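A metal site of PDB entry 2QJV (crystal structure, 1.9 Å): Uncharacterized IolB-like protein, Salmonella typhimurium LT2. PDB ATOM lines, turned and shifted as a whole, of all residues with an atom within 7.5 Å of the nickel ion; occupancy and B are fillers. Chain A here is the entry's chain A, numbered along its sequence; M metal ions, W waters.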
ATOM      1  N   SER A 167     -31.676  14.013  17.291  1.00  0.00           N
ATOM      2  CA  SER A 167     -31.852  15.425  17.654  1.00  0.00           C
ATOM      3  C   SER A 167     -33.023  15.485  18.690  1.00  0.00           C
ATOM      4  O   SER A 167     -33.863  16.379  18.706  1.00  0.00           O
ATOM      5  CB  SER A 167     -32.068  16.319  16.425  1.00  0.00           C
ATOM      6  OG  SER A 167     -30.950  16.152  15.527  1.00  0.00           O
ATOM      7  N   HIS A 171     -34.134  19.886  21.431  1.00  0.00           N
ATOM      8  CA  HIS A 171     -33.254  20.965  21.957  1.00  0.00           C
ATOM      9  C   HIS A 171     -33.344  22.165  21.020  1.00  0.00           C
ATOM     10  O   HIS A 171     -33.708  21.994  19.867  1.00  0.00           O
ATOM     11  CB  HIS A 171     -31.810  20.505  22.101  1.00  0.00           C
ATOM     12  CG  HIS A 171     -31.071  20.307  20.814  1.00  0.00           C
ATOM     13  ND1 HIS A 171     -30.650  19.065  20.382  1.00  0.00           N
ATOM     14  CD2 HIS A 171     -30.640  21.196  19.889  1.00  0.00           C
ATOM     15  CE1 HIS A 171     -30.008  19.200  19.232  1.00  0.00           C
ATOM     16  NE2 HIS A 171     -29.981  20.481  18.914  1.00  0.00           N
ATOM     17  N   MLY A 172     -33.040  23.349  21.531  1.00  0.00           N
ATOM     18  CA  MLY A 172     -32.958  24.577  20.723  1.00  0.00           C
ATOM     19  CB  MLY A 172     -34.190  25.497  20.881  1.00  0.00           C
ATOM     20  CG  MLY A 172     -34.342  26.111  22.283  1.00  0.00           C
ATOM     21  CD  MLY A 172     -35.631  26.910  22.420  1.00  0.00           C
ATOM     22  CE  MLY A 172     -35.771  27.487  23.803  1.00  0.00           C
ATOM     23  NZ  MLY A 172     -34.820  28.526  24.255  1.00  0.00           N
ATOM     24  CH1 MLY A 172     -34.883  29.736  23.389  1.00  0.00           C
ATOM     25  CH2 MLY A 172     -35.178  28.891  25.642  1.00  0.00           C
ATOM     26  C   MLY A 172     -31.669  25.314  21.078  1.00  0.00           C
ATOM     27  O   MLY A 172     -31.137  25.230  22.214  1.00  0.00           O
ATOM     28  N   HIS A 173     -31.187  26.059  20.094  1.00  0.00           N
ATOM     29  CA  HIS A 173     -29.988  26.907  20.183  1.00  0.00           C
ATOM     30  C   HIS A 173     -30.285  28.084  19.248  1.00  0.00           C
ATOM     31  O   HIS A 173     -29.682  28.233  18.175  1.00  0.00           O
ATOM     32  CB  HIS A 173     -28.671  26.160  19.866  1.00  0.00           C
ATOM     33  CG  HIS A 173     -28.825  25.136  18.804  1.00  0.00           C
ATOM     34  ND1 HIS A 173     -29.079  25.459  17.483  1.00  0.00           N
ATOM     35  CD2 HIS A 173     -28.815  23.796  18.868  1.00  0.00           C
ATOM     36  CE1 HIS A 173     -29.239  24.350  16.796  1.00  0.00           C
ATOM     37  NE2 HIS A 173     -29.092  23.327  17.611  1.00  0.00           N
ATOM     38  N   LEU A 184     -27.353  29.572  17.242  1.00  0.00           N
ATOM     39  CA  LEU A 184     -26.642  28.788  16.248  1.00  0.00           C
ATOM     40  C   LEU A 184     -27.587  28.359  15.157  1.00  0.00           C
ATOM     41  O   LEU A 184     -28.558  27.643  15.373  1.00  0.00           O
ATOM     42  CB  LEU A 184     -25.956  27.540  16.864  1.00  0.00           C
ATOM     43  CG  LEU A 184     -24.782  27.774  17.813  1.00  0.00           C
ATOM     44  CD1 LEU A 184     -24.478  26.466  18.479  1.00  0.00           C
ATOM     45  CD2 LEU A 184     -23.452  28.429  17.181  1.00  0.00           C
ATOM     46  N   GLU A 185     -27.342  28.894  13.951  1.00  0.00           N
ATOM     47  CA  GLU A 185     -28.053  28.430  12.778  1.00  0.00           C
ATOM     48  C   GLU A 185     -27.592  26.983  12.543  1.00  0.00           C
ATOM     49  O   GLU A 185     -26.459  26.648  12.851  1.00  0.00           O
ATOM     50  CB  GLU A 185     -27.711  29.309  11.578  1.00  0.00           C
ATOM     51  CG  GLU A 185     -28.218  30.734  11.734  1.00  0.00           C
ATOM     52  CD  GLU A 185     -27.397  31.782  11.015  1.00  0.00           C
ATOM     53  OE1 GLU A 185     -26.501  31.435  10.220  1.00  0.00           O
ATOM     54  OE2 GLU A 185     -27.649  32.981  11.260  1.00  0.00           O
ATOM     55  N   GLU A 186     -28.452  26.155  11.993  1.00  0.00           N
ATOM     56  CA  GLU A 186     -28.103  24.754  11.757  1.00  0.00           C
ATOM     57  C   GLU A 186     -28.706  24.230  10.441  1.00  0.00           C
ATOM     58  O   GLU A 186     -29.867  24.478  10.100  1.00  0.00           O
ATOM     59  CB  GLU A 186     -28.501  23.860  12.944  1.00  0.00           C
ATOM     60  CG  GLU A 186     -27.992  22.431  12.817  1.00  0.00           C
ATOM     61  CD  GLU A 186     -28.107  21.598  14.067  1.00  0.00           C
ATOM     62  OE1 GLU A 186     -28.908  21.945  14.970  1.00  0.00           O
ATOM     63  OE2 GLU A 186     -27.449  20.535  14.152  1.00  0.00           O
ATOM     64  N   TYR A 188     -29.062  20.556   8.080  1.00  0.00           N
ATOM     65  CA  TYR A 188     -29.104  19.099   8.067  1.00  0.00           C
ATOM     66  C   TYR A 188     -29.019  18.693   6.597  1.00  0.00           C
ATOM     67  O   TYR A 188     -29.842  19.123   5.818  1.00  0.00           O
ATOM     68  CB  TYR A 188     -30.432  18.535   8.597  1.00  0.00           C
ATOM     69  CG  TYR A 188     -30.531  18.440  10.112  1.00  0.00           C
ATOM     70  CD1 TYR A 188     -30.541  19.595  10.881  1.00  0.00           C
ATOM     71  CD2 TYR A 188     -30.623  17.209  10.770  1.00  0.00           C
ATOM     72  CE1 TYR A 188     -30.610  19.531  12.242  1.00  0.00           C
ATOM     73  CE2 TYR A 188     -30.688  17.151  12.139  1.00  0.00           C
ATOM     74  CZ  TYR A 188     -30.697  18.316  12.873  1.00  0.00           C
ATOM     75  OH  TYR A 188     -30.769  18.233  14.210  1.00  0.00           O
ATOM     76  N   VAL A 224     -32.578  25.014   9.957  1.00  0.00           N
ATOM     77  CA  VAL A 224     -33.117  25.208  11.302  1.00  0.00           C
ATOM     78  C   VAL A 224     -32.755  26.632  11.778  1.00  0.00           C
ATOM     79  O   VAL A 224     -31.704  26.863  12.413  1.00  0.00           O
ATOM     80  CB  VAL A 224     -32.618  24.129  12.318  1.00  0.00           C
ATOM     81  CG1 VAL A 224     -33.294  24.342  13.667  1.00  0.00           C
ATOM     82  CG2 VAL A 224     -32.830  22.673  11.800  1.00  0.00           C
ATOM     83  N   GLY A 227     -35.877  27.172  16.987  1.00  0.00           N
ATOM     84  CA  GLY A 227     -36.673  26.100  17.565  1.00  0.00           C
ATOM     85  C   GLY A 227     -36.029  24.719  17.729  1.00  0.00           C
ATOM     86  O   GLY A 227     -34.826  24.461  17.400  1.00  0.00           O
ATOM     87  N   TYR A 228     -36.888  23.848  18.217  1.00  0.00           N
ATOM     88  CA  TYR A 228     -36.655  22.388  18.380  1.00  0.00           C
ATOM     89  C   TYR A 228     -36.662  21.771  17.008  1.00  0.00           C
ATOM     90  O   TYR A 228     -37.337  22.269  16.109  1.00  0.00           O
ATOM     91  CB  TYR A 228     -37.723  21.783  19.304  1.00  0.00           C
ATOM     92  CG  TYR A 228     -37.799  22.534  20.628  1.00  0.00           C
ATOM     93  CD1 TYR A 228     -36.736  22.495  21.517  1.00  0.00           C
ATOM     94  CD2 TYR A 228     -38.933  23.287  20.992  1.00  0.00           C
ATOM     95  CE1 TYR A 228     -36.763  23.187  22.673  1.00  0.00           C
ATOM     96  CE2 TYR A 228     -38.956  23.985  22.156  1.00  0.00           C
ATOM     97  CZ  TYR A 228     -37.876  23.923  23.013  1.00  0.00           C
ATOM     98  OH  TYR A 228     -37.878  24.590  24.199  1.00  0.00           O
ATOM     99  N   HIS A 229     -35.899  20.693  16.828  1.00  0.00           N
ATOM    100  CA  HIS A 229     -35.738  20.125  15.481  1.00  0.00           C
ATOM    101  C   HIS A 229     -35.462  18.608  15.427  1.00  0.00           C
ATOM    102  O   HIS A 229     -34.498  18.144  14.755  1.00  0.00           O
ATOM    103  CB  HIS A 229     -34.652  20.930  14.727  1.00  0.00           C
ATOM    104  CG  HIS A 229     -33.451  21.284  15.556  1.00  0.00           C
ATOM    105  ND1 HIS A 229     -33.449  22.346  16.447  1.00  0.00           N
ATOM    106  CD2 HIS A 229     -32.214  20.762  15.611  1.00  0.00           C
ATOM    107  CE1 HIS A 229     -32.267  22.464  16.986  1.00  0.00           C
ATOM    108  NE2 HIS A 229     -31.498  21.512  16.509  1.00  0.00           N
ATOM    109  N   ASN A 243     -24.381  17.901   9.723  1.00  0.00           N
ATOM    110  CA  ASN A 243     -24.809  19.209  10.258  1.00  0.00           C
ATOM    111  C   ASN A 243     -23.704  20.214  10.289  1.00  0.00           C
ATOM    112  O   ASN A 243     -22.545  19.891  10.576  1.00  0.00           O
ATOM    113  CB  ASN A 243     -25.316  19.136  11.730  1.00  0.00           C
ATOM    114  CG  ASN A 243     -26.491  18.190  11.969  1.00  0.00           C
ATOM    115  OD1 ASN A 243     -26.445  17.376  12.891  1.00  0.00           O
ATOM    116  ND2 ASN A 243     -27.498  18.285  11.184  1.00  0.00           N
ATOM    117  N   MET A 245     -23.168  24.175  11.971  1.00  0.00           N
ATOM    118  CA  MET A 245     -23.627  25.237  12.846  1.00  0.00           C
ATOM    119  C   MET A 245     -22.629  26.370  12.922  1.00  0.00           C
ATOM    120  O   MET A 245     -21.428  26.166  12.780  1.00  0.00           O
ATOM    121  CB  MET A 245     -23.887  24.743  14.280  1.00  0.00           C
ATOM    122  CG  MET A 245     -25.092  23.850  14.421  1.00  0.00           C
ATOM    123  SD  MET A 245     -25.256  23.335  16.319  1.00  0.00           S
ATOM    124  CE  MET A 245     -23.750  22.281  16.441  1.00  0.00           C
ATOM    125  N   TRP A 252     -21.454  25.381  21.718  1.00  0.00           N
ATOM    126  CA  TRP A 252     -22.683  24.607  21.541  1.00  0.00           C
ATOM    127  C   TRP A 252     -23.369  24.549  22.897  1.00  0.00           C
ATOM    128  O   TRP A 252     -22.980  23.767  23.766  1.00  0.00           O
ATOM    129  CB  TRP A 252     -22.405  23.201  20.965  1.00  0.00           C
ATOM    130  CG  TRP A 252     -23.663  22.409  20.644  1.00  0.00           C
ATOM    131  CD1 TRP A 252     -24.767  22.850  19.948  1.00  0.00           C
ATOM    132  CD2 TRP A 252     -23.910  21.028  20.932  1.00  0.00           C
ATOM    133  NE1 TRP A 252     -25.699  21.847  19.829  1.00  0.00           N
ATOM    134  CE2 TRP A 252     -25.205  20.717  20.423  1.00  0.00           C
ATOM    135  CE3 TRP A 252     -23.187  20.022  21.601  1.00  0.00           C
ATOM    136  CZ2 TRP A 252     -25.787  19.434  20.552  1.00  0.00           C
ATOM    137  CZ3 TRP A 252     -23.764  18.729  21.721  1.00  0.00           C
ATOM    138  CH2 TRP A 252     -25.052  18.457  21.195  1.00  0.00           C
ATOM    139  N   PHE A 254     -27.316  24.566  24.463  1.00  0.00           N
ATOM    140  CA  PHE A 254     -28.712  24.423  24.061  1.00  0.00           C
ATOM    141  C   PHE A 254     -29.610  24.288  25.262  1.00  0.00           C
ATOM    142  O   PHE A 254     -29.161  24.070  26.413  1.00  0.00           O
ATOM    143  CB  PHE A 254     -28.850  23.219  23.073  1.00  0.00           C
ATOM    144  CG  PHE A 254     -28.386  21.913  23.645  1.00  0.00           C
ATOM    145  CD1 PHE A 254     -29.190  21.201  24.573  1.00  0.00           C
ATOM    146  CD2 PHE A 254     -27.116  21.396  23.326  1.00  0.00           C
ATOM    147  CE1 PHE A 254     -28.752  19.989  25.159  1.00  0.00           C
ATOM    148  CE2 PHE A 254     -26.666  20.185  23.918  1.00  0.00           C
ATOM    149  CZ  PHE A 254     -27.480  19.479  24.834  1.00  0.00           C
HETATM  150 NI    NI M   1     -29.364  21.304  16.918  1.00  0.00          NI
HETATM  151  O   HOH W   1     -29.143  19.287  16.104  1.00  0.00           O
HETATM  152  O   HOH W   2     -27.262  20.938  17.386  1.00  0.00           O
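The backbone carbonyl oxygen (O) of His 173 lies within hydrogen-bond range of the backbone NH (N) of Leu 184, at 2.8 Å. The backbone NH of Val 224 lies within hydrogen-bond range of the backbone carbonyl oxygen of Glu 186, 2.8 Å away. A ring nitrogen (ND1) of His 229 sits at hydrogen-bond distance from the backbone carbonyl oxygen (O) of Gly 227 (2.7 Å).
Water W1 bridges OH of Tyr 188 (2.7 Å) and OE2 of Glu 186 (2.9 Å). Water W2 lies within hydrogen-bond range of the indole nitrogen of Trp 252 (3.0 Å), the side-chain carboxylate of Glu 186 (3.3 Å) and the side-chain sulfur of Met 245 (3.3 Å).
Within 4 Å of the nickel ion: His 171, His 173, Glu 186 and His 229. The nearest printed residue that does not touch the nickel ion is Tyr 188 (4.3 Å).
The nickel ion is bound by the side-chain carboxylate (OE1) of Glu 186 (2.1 Å), a ring nitrogen (NE2) of His 173 (2.2 Å), a ring nitrogen (NE2) of His 229 (2.2 Å), water W2 (2.2 Å), water W1 (2.2 Å) and a ring nitrogen (NE2) of His 171 (2.2 Å). The nickel ion has six donor atoms within binding distance.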
